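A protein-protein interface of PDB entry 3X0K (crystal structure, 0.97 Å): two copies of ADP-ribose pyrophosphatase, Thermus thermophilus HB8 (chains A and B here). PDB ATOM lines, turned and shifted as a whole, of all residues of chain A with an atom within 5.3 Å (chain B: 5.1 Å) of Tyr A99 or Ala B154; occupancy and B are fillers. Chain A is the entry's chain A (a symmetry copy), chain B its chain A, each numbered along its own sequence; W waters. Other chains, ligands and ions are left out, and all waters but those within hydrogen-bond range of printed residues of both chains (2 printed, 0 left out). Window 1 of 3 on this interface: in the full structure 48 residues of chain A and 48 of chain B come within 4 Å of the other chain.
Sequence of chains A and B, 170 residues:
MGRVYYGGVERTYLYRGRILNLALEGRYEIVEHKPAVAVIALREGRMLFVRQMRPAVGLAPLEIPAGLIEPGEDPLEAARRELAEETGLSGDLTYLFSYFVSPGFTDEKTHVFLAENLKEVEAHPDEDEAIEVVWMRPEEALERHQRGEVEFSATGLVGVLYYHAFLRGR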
ATOM      1  N   PHE A  97      33.351 -17.914  -5.104  1.00  0.00           N
ATOM      2  CA  PHE A  97      32.897 -18.946  -6.029  1.00  0.00           C
ATOM      3  C   PHE A  97      31.698 -18.368  -6.776  1.00  0.00           C
ATOM      4  O   PHE A  97      31.208 -17.275  -6.434  1.00  0.00           O
ATOM      5  CB  PHE A  97      32.544 -20.261  -5.311  1.00  0.00           C
ATOM      6  CG  PHE A  97      31.850 -20.120  -3.968  1.00  0.00           C
ATOM      7  CD1 PHE A  97      32.442 -20.664  -2.821  1.00  0.00           C
ATOM      8  CD2 PHE A  97      30.618 -19.473  -3.853  1.00  0.00           C
ATOM      9  CE1 PHE A  97      31.831 -20.524  -1.601  1.00  0.00           C
ATOM     10  CE2 PHE A  97      30.018 -19.316  -2.635  1.00  0.00           C
ATOM     11  CZ  PHE A  97      30.613 -19.853  -1.449  1.00  0.00           C
ATOM     12  N   SER A  98      31.237 -19.119  -7.762  1.00  0.00           N
ATOM     13  CA  SER A  98      30.072 -18.703  -8.548  1.00  0.00           C
ATOM     14  C   SER A  98      29.144 -19.875  -8.726  1.00  0.00           C
ATOM     15  O   SER A  98      29.514 -21.035  -8.552  1.00  0.00           O
ATOM     16  CB  SER A  98      30.521 -18.190  -9.926  1.00  0.00           C
ATOM     17  OG  SER A  98      31.069 -19.279 -10.680  1.00  0.00           O
ATOM     18  N   TYR A  99      27.905 -19.565  -9.139  1.00  0.00           N
ATOM     19  CA  TYR A  99      26.969 -20.625  -9.443  1.00  0.00           C
ATOM     20  C   TYR A  99      25.941 -20.122 -10.430  1.00  0.00           C
ATOM     21  O   TYR A  99      25.558 -18.953 -10.452  1.00  0.00           O
ATOM     22  CB  TYR A  99      26.269 -21.162  -8.165  1.00  0.00           C
ATOM     23  CG  TYR A  99      25.390 -20.159  -7.456  1.00  0.00           C
ATOM     24  CD1 TYR A  99      25.925 -19.267  -6.515  1.00  0.00           C
ATOM     25  CD2 TYR A  99      24.033 -20.079  -7.711  1.00  0.00           C
ATOM     26  CE1 TYR A  99      25.094 -18.347  -5.872  1.00  0.00           C
ATOM     27  CE2 TYR A  99      23.220 -19.183  -7.075  1.00  0.00           C
ATOM     28  CZ  TYR A  99      23.729 -18.318  -6.147  1.00  0.00           C
ATOM     29  OH  TYR A  99      22.976 -17.382  -5.493  1.00  0.00           O
ATOM     30  N   PHE A 100      25.442 -21.072 -11.229  1.00  0.00           N
ATOM     31  CA  PHE A 100      24.258 -20.825 -12.065  1.00  0.00           C
ATOM     32  C   PHE A 100      23.014 -21.039 -11.253  1.00  0.00           C
ATOM     33  O   PHE A 100      22.820 -22.105 -10.652  1.00  0.00           O
ATOM     34  CB  PHE A 100      24.259 -21.764 -13.282  1.00  0.00           C
ATOM     35  CG  PHE A 100      25.341 -21.400 -14.274  1.00  0.00           C
ATOM     36  CD1 PHE A 100      26.450 -22.188 -14.447  1.00  0.00           C
ATOM     37  CD2 PHE A 100      25.212 -20.259 -15.049  1.00  0.00           C
ATOM     38  CE1 PHE A 100      27.447 -21.824 -15.405  1.00  0.00           C
ATOM     39  CE2 PHE A 100      26.172 -19.936 -15.993  1.00  0.00           C
ATOM     40  CZ  PHE A 100      27.250 -20.698 -16.176  1.00  0.00           C
ATOM     41  N   VAL A 101      22.137 -20.019 -11.192  1.00  0.00           N
ATOM     42  CA  VAL A 101      20.991 -20.076 -10.267  1.00  0.00           C
ATOM     43  C   VAL A 101      20.040 -21.223 -10.597  1.00  0.00           C
ATOM     44  O   VAL A 101      19.436 -21.784  -9.667  1.00  0.00           O
ATOM     45  CB  VAL A 101      20.166 -18.762 -10.177  1.00  0.00           C
ATOM     46  CG1 VAL A 101      21.106 -17.578  -9.939  1.00  0.00           C
ATOM     47  CG2 VAL A 101      19.377 -18.515 -11.457  1.00  0.00           C
ATOM     48  N   PRO A 103      20.193 -23.639 -14.033  1.00  0.00           N
ATOM     49  CA  PRO A 103      20.704 -23.753 -15.408  1.00  0.00           C
ATOM     50  C   PRO A 103      19.804 -24.587 -16.320  1.00  0.00           C
ATOM     51  O   PRO A 103      20.099 -24.668 -17.498  1.00  0.00           O
ATOM     52  CB  PRO A 103      22.087 -24.356 -15.250  1.00  0.00           C
ATOM     53  CG  PRO A 103      21.977 -25.167 -13.948  1.00  0.00           C
ATOM     54  CD  PRO A 103      21.111 -24.296 -13.051  1.00  0.00           C
ATOM     55  N   GLU A 108      21.438 -17.123 -15.786  1.00  0.00           N
ATOM     56  CA  GLU A 108      21.902 -16.223 -14.716  1.00  0.00           C
ATOM     57  C   GLU A 108      22.983 -16.910 -13.912  1.00  0.00           C
ATOM     58  O   GLU A 108      22.767 -18.011 -13.368  1.00  0.00           O
ATOM     59  CB  GLU A 108      20.770 -15.802 -13.802  1.00  0.00           C
ATOM     60  CG  GLU A 108      21.229 -14.757 -12.791  1.00  0.00           C
ATOM     61  CD  GLU A 108      20.172 -14.350 -11.799  1.00  0.00           C
ATOM     62  OE1 GLU A 108      19.202 -15.055 -11.605  1.00  0.00           O
ATOM     63  OE2 GLU A 108      20.387 -13.233 -11.220  1.00  0.00           O
ATOM     64  N   LYS A 109      24.112 -16.221 -13.746  1.00  0.00           N
ATOM     65  CA  LYS A 109      25.247 -16.690 -12.993  1.00  0.00           C
ATOM     66  C   LYS A 109      25.486 -15.687 -11.869  1.00  0.00           C
ATOM     67  O   LYS A 109      25.518 -14.475 -12.157  1.00  0.00           O
ATOM     68  CB  LYS A 109      26.471 -16.808 -13.894  1.00  0.00           C
ATOM     69  CG  LYS A 109      27.637 -17.519 -13.247  1.00  0.00           C
ATOM     70  CD  LYS A 109      28.819 -17.623 -14.218  1.00  0.00           C
ATOM     71  CE  LYS A 109      29.708 -18.788 -13.820  1.00  0.00           C
ATOM     72  NZ  LYS A 109      30.904 -18.860 -14.748  1.00  0.00           N
ATOM     73  N   THR A 110      25.706 -16.165 -10.659  1.00  0.00           N
ATOM     74  CA  THR A 110      25.966 -15.339  -9.490  1.00  0.00           C
ATOM     75  C   THR A 110      27.393 -15.531  -9.021  1.00  0.00           C
ATOM     76  O   THR A 110      27.817 -16.671  -8.808  1.00  0.00           O
ATOM     77  CB  THR A 110      24.999 -15.673  -8.369  1.00  0.00           C
ATOM     78  OG1 THR A 110      23.634 -15.518  -8.883  1.00  0.00           O
ATOM     79  CG2 THR A 110      25.132 -14.763  -7.182  1.00  0.00           C
ATOM     80  N   HIS A 111      28.090 -14.420  -8.809  1.00  0.00           N
ATOM     81  CA  HIS A 111      29.456 -14.421  -8.295  1.00  0.00           C
ATOM     82  C   HIS A 111      29.418 -13.968  -6.835  1.00  0.00           C
ATOM     83  O   HIS A 111      28.870 -12.899  -6.560  1.00  0.00           O
ATOM     84  CB  HIS A 111      30.298 -13.429  -9.094  1.00  0.00           C
ATOM     85  CG  HIS A 111      30.307 -13.718 -10.558  1.00  0.00           C
ATOM     86  ND1 HIS A 111      31.255 -14.487 -11.100  1.00  0.00           N
ATOM     87  CD2 HIS A 111      29.439 -13.345 -11.518  1.00  0.00           C
ATOM     88  CE1 HIS A 111      31.012 -14.570 -12.432  1.00  0.00           C
ATOM     89  NE2 HIS A 111      29.928 -13.866 -12.702  1.00  0.00           N
ATOM     90  N   VAL A 112      29.957 -14.798  -5.950  1.00  0.00           N
ATOM     91  CA  VAL A 112      29.833 -14.571  -4.514  1.00  0.00           C
ATOM     92  C   VAL A 112      31.166 -14.127  -3.949  1.00  0.00           C
ATOM     93  O   VAL A 112      32.212 -14.725  -4.226  1.00  0.00           O
ATOM     94  CB  VAL A 112      29.342 -15.860  -3.803  1.00  0.00           C
ATOM     95  CG1 VAL A 112      29.062 -15.548  -2.329  1.00  0.00           C
ATOM     96  CG2 VAL A 112      28.072 -16.382  -4.465  1.00  0.00           C
ATOM     97  N   ALA A 154      18.453 -18.164  -2.725  1.00  0.00           N
ATOM     98  CA  ALA A 154      19.703 -18.914  -2.878  1.00  0.00           C
ATOM     99  C   ALA A 154      20.860 -18.161  -2.235  1.00  0.00           C
ATOM    100  O   ALA A 154      21.710 -18.778  -1.584  1.00  0.00           O
ATOM    101  CB  ALA A 154      19.989 -19.190  -4.326  1.00  0.00           C
ATOM    102  N   THR A 155      20.925 -16.850  -2.449  1.00  0.00           N
ATOM    103  CA  THR A 155      22.092 -16.123  -1.887  1.00  0.00           C
ATOM    104  C   THR A 155      22.080 -16.179  -0.369  1.00  0.00           C
ATOM    105  O   THR A 155      23.135 -16.343   0.252  1.00  0.00           O
ATOM    106  CB  THR A 155      22.143 -14.676  -2.403  1.00  0.00           C
ATOM    107  OG1 THR A 155      20.963 -13.972  -1.971  1.00  0.00           O
ATOM    108  CG2 THR A 155      22.322 -14.593  -3.907  1.00  0.00           C
ATOM    109  N   VAL A 158      23.134 -19.731   0.686  1.00  0.00           N
ATOM    110  CA  VAL A 158      24.586 -19.892   0.463  1.00  0.00           C
ATOM    111  C   VAL A 158      25.352 -19.170   1.534  1.00  0.00           C
ATOM    112  O   VAL A 158      26.329 -19.706   2.056  1.00  0.00           O
ATOM    113  CB  VAL A 158      24.928 -19.390  -0.968  1.00  0.00           C
ATOM    114  CG1 VAL A 158      26.427 -19.139  -1.113  1.00  0.00           C
ATOM    115  CG2 VAL A 158      24.432 -20.392  -2.005  1.00  0.00           C
ATOM    116  N   TYR B  99      14.831 -22.948  -0.893  1.00  0.00           N
ATOM    117  CA  TYR B  99      15.263 -21.623  -1.279  1.00  0.00           C
ATOM    118  C   TYR B  99      14.613 -21.242  -2.589  1.00  0.00           C
ATOM    119  O   TYR B  99      14.343 -22.067  -3.461  1.00  0.00           O
ATOM    120  CB  TYR B  99      16.809 -21.531  -1.399  1.00  0.00           C
ATOM    121  CG  TYR B  99      17.411 -22.389  -2.488  1.00  0.00           C
ATOM    122  CD1 TYR B  99      17.734 -23.733  -2.252  1.00  0.00           C
ATOM    123  CD2 TYR B  99      17.660 -21.884  -3.751  1.00  0.00           C
ATOM    124  CE1 TYR B  99      18.290 -24.507  -3.274  1.00  0.00           C
ATOM    125  CE2 TYR B  99      18.209 -22.642  -4.746  1.00  0.00           C
ATOM    126  CZ  TYR B  99      18.541 -23.950  -4.524  1.00  0.00           C
ATOM    127  OH  TYR B  99      19.071 -24.769  -5.483  1.00  0.00           O
ATOM    128  N   PHE B 152      29.406 -24.616 -11.107  1.00  0.00           N
ATOM    129  CA  PHE B 152      28.392 -25.143 -10.221  1.00  0.00           C
ATOM    130  C   PHE B 152      27.014 -24.670 -10.655  1.00  0.00           C
ATOM    131  O   PHE B 152      26.864 -23.532 -11.046  1.00  0.00           O
ATOM    132  CB  PHE B 152      28.553 -24.650  -8.799  1.00  0.00           C
ATOM    133  CG  PHE B 152      29.601 -25.381  -7.969  1.00  0.00           C
ATOM    134  CD1 PHE B 152      30.627 -24.689  -7.362  1.00  0.00           C
ATOM    135  CD2 PHE B 152      29.469 -26.755  -7.752  1.00  0.00           C
ATOM    136  CE1 PHE B 152      31.546 -25.370  -6.560  1.00  0.00           C
ATOM    137  CE2 PHE B 152      30.352 -27.419  -6.953  1.00  0.00           C
ATOM    138  CZ  PHE B 152      31.398 -26.735  -6.346  1.00  0.00           C
ATOM    139  N   SER B 153      26.007 -25.533 -10.457  1.00  0.00           N
ATOM    140  CA  SER B 153      24.655 -25.006 -10.281  1.00  0.00           C
ATOM    141  C   SER B 153      24.483 -24.619  -8.795  1.00  0.00           C
ATOM    142  O   SER B 153      25.239 -25.045  -7.932  1.00  0.00           O
ATOM    143  CB  SER B 153      23.618 -26.026 -10.666  1.00  0.00           C
ATOM    144  OG  SER B 153      23.647 -27.113  -9.723  1.00  0.00           O
ATOM    145  N   ALA B 154      23.391 -23.880  -8.529  1.00  0.00           N
ATOM    146  CA  ALA B 154      23.051 -23.609  -7.128  1.00  0.00           C
ATOM    147  C   ALA B 154      22.935 -24.911  -6.347  1.00  0.00           C
ATOM    148  O   ALA B 154      23.395 -24.984  -5.202  1.00  0.00           O
ATOM    149  CB  ALA B 154      21.781 -22.815  -7.029  1.00  0.00           C
ATOM    150  N   THR B 155      22.287 -25.914  -6.930  1.00  0.00           N
ATOM    151  CA  THR B 155      22.105 -27.160  -6.143  1.00  0.00           C
ATOM    152  C   THR B 155      23.448 -27.805  -5.840  1.00  0.00           C
ATOM    153  O   THR B 155      23.656 -28.307  -4.731  1.00  0.00           O
ATOM    154  CB  THR B 155      21.155 -28.134  -6.859  1.00  0.00           C
ATOM    155  OG1 THR B 155      21.727 -28.518  -8.124  1.00  0.00           O
ATOM    156  CG2 THR B 155      19.756 -27.574  -7.027  1.00  0.00           C
ATOM    157  N   GLY B 156      24.378 -27.812  -6.816  1.00  0.00           N
ATOM    158  CA  GLY B 156      25.698 -28.387  -6.572  1.00  0.00           C
ATOM    159  C   GLY B 156      26.454 -27.642  -5.475  1.00  0.00           C
ATOM    160  O   GLY B 156      27.078 -28.258  -4.601  1.00  0.00           O
ATOM    161  N   LEU B 157      26.436 -26.310  -5.544  1.00  0.00           N
ATOM    162  CA  LEU B 157      27.119 -25.518  -4.526  1.00  0.00           C
ATOM    163  C   LEU B 157      26.490 -25.706  -3.172  1.00  0.00           C
ATOM    164  O   LEU B 157      27.219 -25.840  -2.166  1.00  0.00           O
ATOM    165  CB  LEU B 157      27.084 -24.020  -4.949  1.00  0.00           C
ATOM    166  CG  LEU B 157      27.709 -23.077  -3.935  1.00  0.00           C
ATOM    167  CD1 LEU B 157      29.200 -23.359  -3.747  1.00  0.00           C
ATOM    168  CD2 LEU B 157      27.498 -21.626  -4.412  1.00  0.00           C
ATOM    169  N   VAL B 158      25.167 -25.713  -3.098  1.00  0.00           N
ATOM    170  CA  VAL B 158      24.495 -25.964  -1.807  1.00  0.00           C
ATOM    171  C   VAL B 158      24.904 -27.305  -1.268  1.00  0.00           C
ATOM    172  O   VAL B 158      25.179 -27.429  -0.075  1.00  0.00           O
ATOM    173  CB  VAL B 158      22.960 -25.837  -2.010  1.00  0.00           C
ATOM    174  CG1 VAL B 158      22.201 -26.478  -0.850  1.00  0.00           C
ATOM    175  CG2 VAL B 158      22.574 -24.371  -2.179  1.00  0.00           C
ATOM    176  N   GLY B 159      24.968 -28.354  -2.117  1.00  0.00           N
ATOM    177  CA  GLY B 159      25.415 -29.648  -1.608  1.00  0.00           C
ATOM    178  C   GLY B 159      26.821 -29.576  -1.021  1.00  0.00           C
ATOM    179  O   GLY B 159      27.095 -30.101   0.041  1.00  0.00           O
HETATM  180  O   HOH W   1      18.802 -24.081  -8.189  1.00  0.00           O
HETATM  181  O   HOH W   2      29.840 -21.827 -11.618  1.00  0.00           O
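The backbone carbonyl oxygen (O) of Phe B152 sits at hydrogen-bond distance from the backbone NH (N) of Phe A100. The backbone carbonyl oxygen of Phe A100 is in hydrogen-bond range of the backbone NH of Ala B154, at 2.8 Å.
OG1 of Thr B155 sits at hydrogen-bond distance from OG of Ser B153 (2.9 Å). The side-chain hydroxyl of Ser B153 sits at hydrogen-bond distance from the backbone NH of Gly B156 (3.1 Å). The backbone carbonyl oxygen of Phe A97 sits at hydrogen-bond distance from the backbone NH of Val A112, 2.8 Å away. The backbone carbonyl oxygen of Tyr A99 is in hydrogen-bond range of the backbone NH of Thr A110 (2.8 Å). The backbone carbonyl oxygen of Glu A108 is in hydrogen-bond range of the backbone NH of Val A101, 3.0 Å away.
Phe A97 touches Leu B157 (CD2 to CD2, 3.8 Å). Phe B152 touches Ser A98 (CB to O, 3.7 Å). Phe B152 touches Tyr A99 (O to CA, 3.3 Å). C of Ser B153 touches CB of Tyr A99, at 3.9 Å. Tyr A99 touches Ala B154. Leu B157 touches Tyr A99 (CD2 to CD1, 3.5 Å). Phe A100 touches Ser B153. Val A101 touches Ala B154 (O to CB, 3.7 Å). Pro A103 touches Ser B153 (CG to CB, 3.8 Å). Ala A154 touches Tyr B99.
Tyr A99 touches just these residues of chain B: Phe B152 (3.3 Å), Ser B153 (3.9 Å), Ala B154 (3.6 Å) and Leu B157 (3.5 Å). Of the printed residues of chain B, Val A101 touches Ala B154. Of the printed residues of chain B, Ala A154 touches Tyr B99 (3.6 Å). Of the printed residues of chain A, Ala B154 touches Tyr A99 (3.6 Å), Phe A100 (2.8 Å) and Val A101 (3.7 Å). The nearest printed residue of chain A that does not touch Ala B154 is Ala A154 (4.9 Å).
Of the 9 printed residues of chain B, 5 touch a printed residue of chain A. Hydrophobic or aromatic side chains of chain A that line the printed part of chain B: Phe A97, Tyr A99, Phe A100, Pro A103 and Ala A154.
Tyr A99 touches Ala B154, and with the chains exchanged Ala A154 touches Tyr B99. 4 positions are printed for both chains. Of the 12 pairs that touch across the chains among the printed residues, 2 have their exchanged pair printed and touching as well.
Water W1 bridges O of Val A101 (2.8 Å) and OH of Tyr B99 (2.8 Å). Water W2 bridges N of Phe B152 (2.9 Å) and OG of Ser A98 (3.0 Å).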
